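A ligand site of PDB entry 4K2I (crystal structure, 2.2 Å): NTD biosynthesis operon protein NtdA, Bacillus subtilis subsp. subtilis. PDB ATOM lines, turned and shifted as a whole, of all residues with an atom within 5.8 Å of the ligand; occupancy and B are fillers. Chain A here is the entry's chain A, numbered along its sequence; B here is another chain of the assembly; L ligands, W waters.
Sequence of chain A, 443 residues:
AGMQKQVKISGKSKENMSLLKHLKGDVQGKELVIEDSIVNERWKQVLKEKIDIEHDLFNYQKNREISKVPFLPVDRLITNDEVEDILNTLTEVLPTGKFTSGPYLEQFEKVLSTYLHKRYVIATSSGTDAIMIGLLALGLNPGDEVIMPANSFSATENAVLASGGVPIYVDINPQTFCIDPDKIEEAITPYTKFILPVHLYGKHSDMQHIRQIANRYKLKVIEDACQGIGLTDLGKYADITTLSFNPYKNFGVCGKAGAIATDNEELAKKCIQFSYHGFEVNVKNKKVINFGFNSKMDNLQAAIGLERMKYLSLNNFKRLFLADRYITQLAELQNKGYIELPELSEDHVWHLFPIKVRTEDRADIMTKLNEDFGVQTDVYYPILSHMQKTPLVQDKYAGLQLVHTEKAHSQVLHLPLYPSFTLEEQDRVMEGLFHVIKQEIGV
The side-chain sulfur (SG) of Cys 226 sits close to the backbone NH (N) of Ser 244 (3.7 Å).
The side-chain carboxylate (OD1) of Asp 224 is in hydrogen-bond range of the backbone NH (N) of Cys 226 (3.0 Å).
The side-chain carboxylate (OD2) of Asp 224 sits at hydrogen-bond distance from the side-chain hydroxyl (OG1) of Thr 156, at 2.8 Å.
The backbone NH (N) of Thr 128 lies close to the side-chain hydroxyl (OG) of Ser 126.
OD2 of Asp 129 is in hydrogen-bond range of OG of Ser 126 (2.7 Å).
The backbone carbonyl oxygen (O) of Phe 153 sits at hydrogen-bond distance from the side-chain hydroxyl (OG1) of Thr 156 (3.4 Å).
The backbone carbonyl oxygen (O) of Ala 257 lies within hydrogen-bond range of the backbone NH (N) of Phe 245, at 2.8 Å.
The side-chain hydroxyl (OG) of Ser 152 lies within hydrogen-bond range of the side-chain hydroxyl (OG1) of Thr 156, at 2.7 Å.
Merely in contact with the ligand: Ser 126, Phe 153, Ala 155, Cys 226, Ala 257, Ser 152 and Thr 156.
Hydrophobic or aromatic side chains within 4 Å of the ligand: Phe 153 and Ala 155.
Within 4 Å of the ligand: Ser 126, Gly 127, Thr 128, Ser 152, Phe 153, Ala 155, Thr 156, Asp 224, Cys 226, Gln 227, Ser 244, Asn 246, Lys 249, Ala 257, Tyr 381 and Asn 294 of chain B.
Along chain A the residues within 4 Å of the ligand span positions 126 to 381.
The nearest printed residue that does not touch the ligand is Val 198 (4.2 Å).
O4 of the ligand lies within hydrogen-bond range of OG of Ser 244 (2.6 Å).
The side-chain carboxylate (OD2) of Asp 224 is in hydrogen-bond range of a nitrogen (N1) of the ligand (2.7 Å).
O3 of the ligand lies within hydrogen-bond range of ND2 of Asn 294 of chain B.
N of Gly 127 is in hydrogen-bond range of O4 of the ligand, at 2.8 Å.
The backbone NH of Thr 128 sits at hydrogen-bond distance from an oxygen (O3) of the ligand.
O3 of the ligand sits at hydrogen-bond distance from OG1 of Thr 128, at 2.9 Å.
An oxygen (O1) of the ligand sits at hydrogen-bond distance from the side-chain amide nitrogen (NE2) of Gln 227, at 2.9 Å.
An oxygen (O5) of the ligand lies within hydrogen-bond range of the side-chain amide nitrogen (ND2) of Asn 246.
The side-chain amino group (NZ) of Lys 249 is in hydrogen-bond range of an oxygen (O1) of the ligand, 3.1 Å away.
The side-chain hydroxyl of Tyr 381 lies within hydrogen-bond range of an oxygen (O1) of the ligand.
Water W3 bridges O4 of the ligand (2.5 Å) and N of Ala 257 (3.2 Å).
Water W2 bridges the side-chain hydroxyl (OH) of Tyr 381 and a nitrogen (N2) of the ligand.
Water W4 lies within hydrogen-bond range of an oxygen (O5) of the ligand, a ring nitrogen (NE2) of His 277 of chain B and the side-chain amide nitrogen of Asn 294 of chain B.
Water W1 bridges an oxygen (O5) of the ligand (2.8 Å) and the side-chain amide nitrogen (ND2) of Asn 294 of chain B (3.2 Å).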
ATOM      1  N   SER A 126     -17.813  35.205  10.481  1.00  0.00           N
ATOM      2  CA  SER A 126     -17.593  33.767  10.654  1.00  0.00           C
ATOM      3  C   SER A 126     -17.253  33.090   9.330  1.00  0.00           C
ATOM      4  O   SER A 126     -17.457  33.667   8.255  1.00  0.00           O
ATOM      5  CB  SER A 126     -18.815  33.078  11.291  1.00  0.00           C
ATOM      6  OG  SER A 126     -19.879  32.985  10.365  1.00  0.00           O
ATOM      7  N   GLY A 127     -16.748  31.870   9.408  1.00  0.00           N
ATOM      8  CA  GLY A 127     -16.493  31.069   8.221  1.00  0.00           C
ATOM      9  C   GLY A 127     -17.775  30.731   7.485  1.00  0.00           C
ATOM     10  O   GLY A 127     -17.791  30.654   6.256  1.00  0.00           O
ATOM     11  N   THR A 128     -18.851  30.526   8.235  1.00  0.00           N
ATOM     12  CA  THR A 128     -20.153  30.224   7.661  1.00  0.00           C
ATOM     13  C   THR A 128     -20.628  31.385   6.797  1.00  0.00           C
ATOM     14  O   THR A 128     -21.133  31.183   5.704  1.00  0.00           O
ATOM     15  CB  THR A 128     -21.219  30.009   8.774  1.00  0.00           C
ATOM     16  OG1 THR A 128     -20.880  28.838   9.533  1.00  0.00           O
ATOM     17  CG2 THR A 128     -22.629  29.843   8.185  1.00  0.00           C
ATOM     18  N   ASP A 129     -20.434  32.589   7.308  1.00  0.00           N
ATOM     19  CA  ASP A 129     -20.774  33.805   6.583  1.00  0.00           C
ATOM     20  C   ASP A 129     -19.890  34.002   5.353  1.00  0.00           C
ATOM     21  O   ASP A 129     -20.372  34.475   4.330  1.00  0.00           O
ATOM     22  CB  ASP A 129     -20.673  35.027   7.513  1.00  0.00           C
ATOM     23  CG  ASP A 129     -21.824  35.101   8.536  1.00  0.00           C
ATOM     24  OD1 ASP A 129     -22.971  35.372   8.123  1.00  0.00           O
ATOM     25  OD2 ASP A 129     -21.576  34.927   9.747  1.00  0.00           O
ATOM     26  N   ILE A 131     -18.613  31.677   3.410  1.00  0.00           N
ATOM     27  CA  ILE A 131     -19.142  30.791   2.387  1.00  0.00           C
ATOM     28  C   ILE A 131     -20.457  31.325   1.813  1.00  0.00           C
ATOM     29  O   ILE A 131     -20.642  31.332   0.601  1.00  0.00           O
ATOM     30  CB  ILE A 131     -19.363  29.348   2.902  1.00  0.00           C
ATOM     31  CG1 ILE A 131     -18.075  28.767   3.479  1.00  0.00           C
ATOM     32  CG2 ILE A 131     -19.918  28.445   1.771  1.00  0.00           C
ATOM     33  CD1 ILE A 131     -18.221  27.375   4.033  1.00  0.00           C
ATOM     34  N   SER A 152     -18.997  16.938   5.710  1.00  0.00           N
ATOM     35  CA  SER A 152     -18.425  18.133   6.328  1.00  0.00           C
ATOM     36  C   SER A 152     -19.243  18.488   7.570  1.00  0.00           C
ATOM     37  O   SER A 152     -20.239  17.834   7.847  1.00  0.00           O
ATOM     38  CB  SER A 152     -18.458  19.314   5.360  1.00  0.00           C
ATOM     39  OG  SER A 152     -17.843  20.443   5.962  1.00  0.00           O
ATOM     40  N   PHE A 153     -18.807  19.525   8.301  1.00  0.00           N
ATOM     41  CA  PHE A 153     -19.591  20.109   9.371  1.00  0.00           C
ATOM     42  C   PHE A 153     -20.818  20.757   8.730  1.00  0.00           C
ATOM     43  O   PHE A 153     -20.738  21.230   7.597  1.00  0.00           O
ATOM     44  CB  PHE A 153     -18.761  21.159  10.148  1.00  0.00           C
ATOM     45  CG  PHE A 153     -19.505  21.837  11.293  1.00  0.00           C
ATOM     46  CD1 PHE A 153     -20.049  21.093  12.335  1.00  0.00           C
ATOM     47  CD2 PHE A 153     -19.613  23.223  11.352  1.00  0.00           C
ATOM     48  CE1 PHE A 153     -20.707  21.721  13.406  1.00  0.00           C
ATOM     49  CE2 PHE A 153     -20.260  23.852  12.387  1.00  0.00           C
ATOM     50  CZ  PHE A 153     -20.815  23.099  13.429  1.00  0.00           C
ATOM     51  N   ALA A 155     -22.188  23.445   8.817  1.00  0.00           N
ATOM     52  CA  ALA A 155     -22.016  24.818   8.359  1.00  0.00           C
ATOM     53  C   ALA A 155     -21.907  24.929   6.836  1.00  0.00           C
ATOM     54  O   ALA A 155     -22.431  25.873   6.246  1.00  0.00           O
ATOM     55  CB  ALA A 155     -20.802  25.456   9.014  1.00  0.00           C
ATOM     56  N   THR A 156     -21.209  23.974   6.207  1.00  0.00           N
ATOM     57  CA  THR A 156     -20.987  24.057   4.770  1.00  0.00           C
ATOM     58  C   THR A 156     -22.315  24.043   4.005  1.00  0.00           C
ATOM     59  O   THR A 156     -22.571  24.962   3.239  1.00  0.00           O
ATOM     60  CB  THR A 156     -20.073  22.919   4.253  1.00  0.00           C
ATOM     61  OG1 THR A 156     -18.968  22.733   5.149  1.00  0.00           O
ATOM     62  CG2 THR A 156     -19.562  23.239   2.858  1.00  0.00           C
ATOM     63  N   VAL A 198     -14.257  20.591   0.188  1.00  0.00           N
ATOM     64  CA  VAL A 198     -13.907  20.844   1.585  1.00  0.00           C
ATOM     65  C   VAL A 198     -12.579  20.195   1.902  1.00  0.00           C
ATOM     66  O   VAL A 198     -12.399  18.987   1.692  1.00  0.00           O
ATOM     67  CB  VAL A 198     -14.978  20.271   2.538  1.00  0.00           C
ATOM     68  CG1 VAL A 198     -14.555  20.469   3.998  1.00  0.00           C
ATOM     69  CG2 VAL A 198     -16.340  20.916   2.251  1.00  0.00           C
ATOM     70  N   LEU A 200     -11.207  18.717   4.322  1.00  0.00           N
ATOM     71  CA  LEU A 200     -11.674  18.148   5.591  1.00  0.00           C
ATOM     72  C   LEU A 200     -10.498  17.703   6.466  1.00  0.00           C
ATOM     73  O   LEU A 200      -9.541  17.112   5.968  1.00  0.00           O
ATOM     74  CB  LEU A 200     -12.618  16.971   5.329  1.00  0.00           C
ATOM     75  CG  LEU A 200     -13.442  16.507   6.538  1.00  0.00           C
ATOM     76  CD1 LEU A 200     -14.263  17.670   7.105  1.00  0.00           C
ATOM     77  CD2 LEU A 200     -14.379  15.343   6.156  1.00  0.00           C
ATOM     78  N   ASP A 224     -14.161  25.418   0.771  1.00  0.00           N
ATOM     79  CA  ASP A 224     -14.250  25.511   2.212  1.00  0.00           C
ATOM     80  C   ASP A 224     -12.904  25.078   2.770  1.00  0.00           C
ATOM     81  O   ASP A 224     -12.634  23.885   2.916  1.00  0.00           O
ATOM     82  CB  ASP A 224     -15.394  24.634   2.723  1.00  0.00           C
ATOM     83  CG  ASP A 224     -15.549  24.680   4.224  1.00  0.00           C
ATOM     84  OD1 ASP A 224     -14.667  25.241   4.909  1.00  0.00           O
ATOM     85  OD2 ASP A 224     -16.564  24.129   4.729  1.00  0.00           O
ATOM     86  N   CYS A 226     -11.953  26.158   5.772  1.00  0.00           N
ATOM     87  CA  CYS A 226     -12.078  26.624   7.155  1.00  0.00           C
ATOM     88  C   CYS A 226     -11.143  25.845   8.117  1.00  0.00           C
ATOM     89  O   CYS A 226     -10.736  26.373   9.155  1.00  0.00           O
ATOM     90  CB  CYS A 226     -13.550  26.633   7.596  1.00  0.00           C
ATOM     91  SG  CYS A 226     -14.566  27.928   6.738  1.00  0.00           S
ATOM     92  N   GLN A 227     -10.767  24.635   7.737  1.00  0.00           N
ATOM     93  CA  GLN A 227      -9.842  23.813   8.522  1.00  0.00           C
ATOM     94  C   GLN A 227      -8.418  23.749   7.954  1.00  0.00           C
ATOM     95  O   GLN A 227      -7.567  23.003   8.452  1.00  0.00           O
ATOM     96  CB  GLN A 227     -10.391  22.369   8.662  1.00  0.00           C
ATOM     97  CG  GLN A 227     -11.659  22.294   9.507  1.00  0.00           C
ATOM     98  CD  GLN A 227     -12.190  20.881   9.700  1.00  0.00           C
ATOM     99  OE1 GLN A 227     -11.568  19.903   9.263  1.00  0.00           O
ATOM    100  NE2 GLN A 227     -13.353  20.753  10.335  1.00  0.00           N
ATOM    101  N   LEU A 243     -12.086  30.878   4.930  1.00  0.00           N
ATOM    102  CA  LEU A 243     -11.421  30.476   6.141  1.00  0.00           C
ATOM    103  C   LEU A 243     -12.326  30.773   7.342  1.00  0.00           C
ATOM    104  O   LEU A 243     -13.219  31.613   7.257  1.00  0.00           O
ATOM    105  CB  LEU A 243     -10.127  31.259   6.328  1.00  0.00           C
ATOM    106  CG  LEU A 243      -9.072  31.239   5.221  1.00  0.00           C
ATOM    107  CD1 LEU A 243      -8.106  32.401   5.431  1.00  0.00           C
ATOM    108  CD2 LEU A 243      -8.316  29.913   5.242  1.00  0.00           C
ATOM    109  N   SER A 244     -12.060  30.075   8.436  1.00  0.00           N
ATOM    110  CA  SER A 244     -12.679  30.337   9.709  1.00  0.00           C
ATOM    111  C   SER A 244     -11.570  30.710  10.676  1.00  0.00           C
ATOM    112  O   SER A 244     -10.496  30.123  10.652  1.00  0.00           O
ATOM    113  CB  SER A 244     -13.390  29.078  10.235  1.00  0.00           C
ATOM    114  OG  SER A 244     -13.806  29.216  11.578  1.00  0.00           O
ATOM    115  N   PHE A 245     -11.833  31.678  11.550  1.00  0.00           N
ATOM    116  CA  PHE A 245     -10.897  31.968  12.626  1.00  0.00           C
ATOM    117  C   PHE A 245     -11.544  31.690  13.988  1.00  0.00           C
ATOM    118  O   PHE A 245     -11.217  32.343  14.967  1.00  0.00           O
ATOM    119  CB  PHE A 245     -10.387  33.412  12.544  1.00  0.00           C
ATOM    120  CG  PHE A 245      -9.865  33.784  11.184  1.00  0.00           C
ATOM    121  CD1 PHE A 245      -8.860  33.042  10.593  1.00  0.00           C
ATOM    122  CD2 PHE A 245     -10.367  34.884  10.506  1.00  0.00           C
ATOM    123  CE1 PHE A 245      -8.369  33.377   9.329  1.00  0.00           C
ATOM    124  CE2 PHE A 245      -9.887  35.233   9.258  1.00  0.00           C
ATOM    125  CZ  PHE A 245      -8.894  34.471   8.658  1.00  0.00           C
ATOM    126  N   ASN A 246     -12.462  30.725  14.045  1.00  0.00           N
ATOM    127  CA  ASN A 246     -13.068  30.412  15.337  1.00  0.00           C
ATOM    128  C   ASN A 246     -12.008  29.843  16.292  1.00  0.00           C
ATOM    129  O   ASN A 246     -10.944  29.387  15.851  1.00  0.00           O
ATOM    130  CB  ASN A 246     -14.377  29.573  15.201  1.00  0.00           C
ATOM    131  CG  ASN A 246     -14.147  28.078  15.053  1.00  0.00           C
ATOM    132  OD1 ASN A 246     -13.230  27.497  15.627  1.00  0.00           O
ATOM    133  ND2 ASN A 246     -15.023  27.435  14.279  1.00  0.00           N
ATOM    134  N   LYS A 249      -9.746  26.631  15.525  1.00  0.00           N
ATOM    135  CA  LYS A 249      -9.006  26.380  14.285  1.00  0.00           C
ATOM    136  C   LYS A 249      -7.494  26.454  14.495  1.00  0.00           C
ATOM    137  O   LYS A 249      -7.037  26.901  15.557  1.00  0.00           O
ATOM    138  CB  LYS A 249      -9.464  27.337  13.188  1.00  0.00           C
ATOM    139  CG  LYS A 249     -10.926  27.229  12.872  1.00  0.00           C
ATOM    140  CD  LYS A 249     -11.335  25.769  12.649  1.00  0.00           C
ATOM    141  CE  LYS A 249     -12.825  25.651  12.347  1.00  0.00           C
ATOM    142  NZ  LYS A 249     -13.316  24.263  12.578  1.00  0.00           N
ATOM    143  N   LYS A 256     -16.092  34.678  17.176  1.00  0.00           N
ATOM    144  CA  LYS A 256     -16.298  34.240  15.801  1.00  0.00           C
ATOM    145  C   LYS A 256     -15.662  35.212  14.798  1.00  0.00           C
ATOM    146  O   LYS A 256     -15.656  36.431  15.018  1.00  0.00           O
ATOM    147  CB  LYS A 256     -17.781  34.076  15.500  1.00  0.00           C
ATOM    148  CG  LYS A 256     -18.471  33.098  16.439  1.00  0.00           C
ATOM    149  CD  LYS A 256     -19.662  32.452  15.781  1.00  0.00           C
ATOM    150  CE  LYS A 256     -20.926  32.871  16.468  1.00  0.00           C
ATOM    151  NZ  LYS A 256     -20.962  34.352  16.508  1.00  0.00           N
ATOM    152  N   ALA A 257     -15.151  34.653  13.705  1.00  0.00           N
ATOM    153  CA  ALA A 257     -14.651  35.405  12.558  1.00  0.00           C
ATOM    154  C   ALA A 257     -14.309  34.448  11.426  1.00  0.00           C
ATOM    155  O   ALA A 257     -14.187  33.234  11.632  1.00  0.00           O
ATOM    156  CB  ALA A 257     -13.416  36.239  12.945  1.00  0.00           C
ATOM    157  N   GLY A 258     -14.163  35.004  10.230  1.00  0.00           N
ATOM    158  CA  GLY A 258     -13.694  34.245   9.084  1.00  0.00           C
ATOM    159  C   GLY A 258     -13.127  35.162   8.013  1.00  0.00           C
ATOM    160  O   GLY A 258     -12.853  36.337   8.282  1.00  0.00           O
ATOM    161  N   HIS A 351      -5.443  19.621  11.197  1.00  0.00           N
ATOM    162  CA  HIS A 351      -6.415  20.186  12.114  1.00  0.00           C
ATOM    163  C   HIS A 351      -7.011  19.053  12.966  1.00  0.00           C
ATOM    164  O   HIS A 351      -7.188  19.202  14.182  1.00  0.00           O
ATOM    165  CB  HIS A 351      -7.499  20.936  11.353  1.00  0.00           C
ATOM    166  CG  HIS A 351      -8.558  21.490  12.249  1.00  0.00           C
ATOM    167  ND1 HIS A 351      -8.309  22.530  13.116  1.00  0.00           N
ATOM    168  CD2 HIS A 351      -9.842  21.124  12.437  1.00  0.00           C
ATOM    169  CE1 HIS A 351      -9.407  22.798  13.792  1.00  0.00           C
ATOM    170  NE2 HIS A 351     -10.353  21.955  13.408  1.00  0.00           N
ATOM    171  N   TYR A 381     -17.779  13.943  11.707  1.00  0.00           N
ATOM    172  CA  TYR A 381     -18.895  14.378  12.526  1.00  0.00           C
ATOM    173  C   TYR A 381     -19.886  13.211  12.638  1.00  0.00           C
ATOM    174  O   TYR A 381     -19.849  12.303  11.822  1.00  0.00           O
ATOM    175  CB  TYR A 381     -19.550  15.609  11.884  1.00  0.00           C
ATOM    176  CG  TYR A 381     -18.552  16.733  11.760  1.00  0.00           C
ATOM    177  CD1 TYR A 381     -17.726  16.831  10.647  1.00  0.00           C
ATOM    178  CD2 TYR A 381     -18.400  17.664  12.779  1.00  0.00           C
ATOM    179  CE1 TYR A 381     -16.770  17.832  10.544  1.00  0.00           C
ATOM    180  CE2 TYR A 381     -17.450  18.684  12.686  1.00  0.00           C
ATOM    181  CZ  TYR A 381     -16.640  18.759  11.557  1.00  0.00           C
ATOM    182  OH  TYR A 381     -15.696  19.752  11.453  1.00  0.00           O
ATOM    183  N   HIS B 277     -27.233  26.758  13.382  1.00  0.00           N
ATOM    184  CA  HIS B 277     -27.104  25.708  12.381  1.00  0.00           C
ATOM    185  C   HIS B 277     -28.301  24.771  12.201  1.00  0.00           C
ATOM    186  O   HIS B 277     -28.175  23.742  11.545  1.00  0.00           O
ATOM    187  CB  HIS B 277     -25.848  24.876  12.634  1.00  0.00           C
ATOM    188  CG  HIS B 277     -24.581  25.634  12.433  1.00  0.00           C
ATOM    189  ND1 HIS B 277     -24.227  26.163  11.205  1.00  0.00           N
ATOM    190  CD2 HIS B 277     -23.596  25.981  13.294  1.00  0.00           C
ATOM    191  CE1 HIS B 277     -23.075  26.798  11.327  1.00  0.00           C
ATOM    192  NE2 HIS B 277     -22.666  26.702  12.578  1.00  0.00           N
ATOM    193  N   ASN B 294     -24.884  30.780  11.929  1.00  0.00           N
ATOM    194  CA  ASN B 294     -23.928  30.768  13.016  1.00  0.00           C
ATOM    195  C   ASN B 294     -24.013  32.135  13.635  1.00  0.00           C
ATOM    196  O   ASN B 294     -23.137  32.991  13.431  1.00  0.00           O
ATOM    197  CB  ASN B 294     -22.519  30.497  12.487  1.00  0.00           C
ATOM    198  CG  ASN B 294     -21.516  30.300  13.606  1.00  0.00           C
ATOM    199  OD1 ASN B 294     -21.891  30.220  14.770  1.00  0.00           O
ATOM    200  ND2 ASN B 294     -20.236  30.221  13.255  1.00  0.00           N
HETATM  201  N1  LIG L   1     -16.541  24.549   7.399  1.00  0.00           N
HETATM  202  C1  LIG L   1     -15.873  23.653   8.219  1.00  0.00           C
HETATM  203  C2  LIG L   1     -15.212  22.423   7.634  1.00  0.00           C
HETATM  204  C3  LIG L   1     -15.811  23.905   9.604  1.00  0.00           C
HETATM  205  O1  LIG L   1     -15.161  23.021  10.433  1.00  0.00           O
HETATM  206  C4  LIG L   1     -16.413  25.037  10.131  1.00  0.00           C
HETATM  207  C5  LIG L   1     -16.360  25.302  11.640  1.00  0.00           C
HETATM  208  N2  LIG L   1     -16.342  24.061  12.429  1.00  0.00           N
HETATM  209  C6  LIG L   1     -17.087  25.921   9.267  1.00  0.00           C
HETATM  210  C7  LIG L   1     -17.142  25.658   7.909  1.00  0.00           C
HETATM  211  C8  LIG L   1     -17.767  27.160   9.782  1.00  0.00           C
HETATM  212  O2  LIG L   1     -16.842  28.064  10.331  1.00  0.00           O
HETATM  213  P1  LIG L   1     -17.303  29.135  11.453  1.00  0.00           P
HETATM  214  O3  LIG L   1     -18.648  29.726  11.108  1.00  0.00           O
HETATM  215  O4  LIG L   1     -16.221  30.210  11.569  1.00  0.00           O
HETATM  216  O5  LIG L   1     -17.486  28.357  12.764  1.00  0.00           O
HETATM  217  O   HOH W   1     -17.790  29.678  15.182  1.00  0.00           O
HETATM  218  O   HOH W   2     -15.846  21.572  13.508  1.00  0.00           O
HETATM  219  O   HOH W   3     -16.332  31.679  13.642  1.00  0.00           O
HETATM  220  O   HOH W   4     -19.862  27.139  13.478  1.00  0.00           O
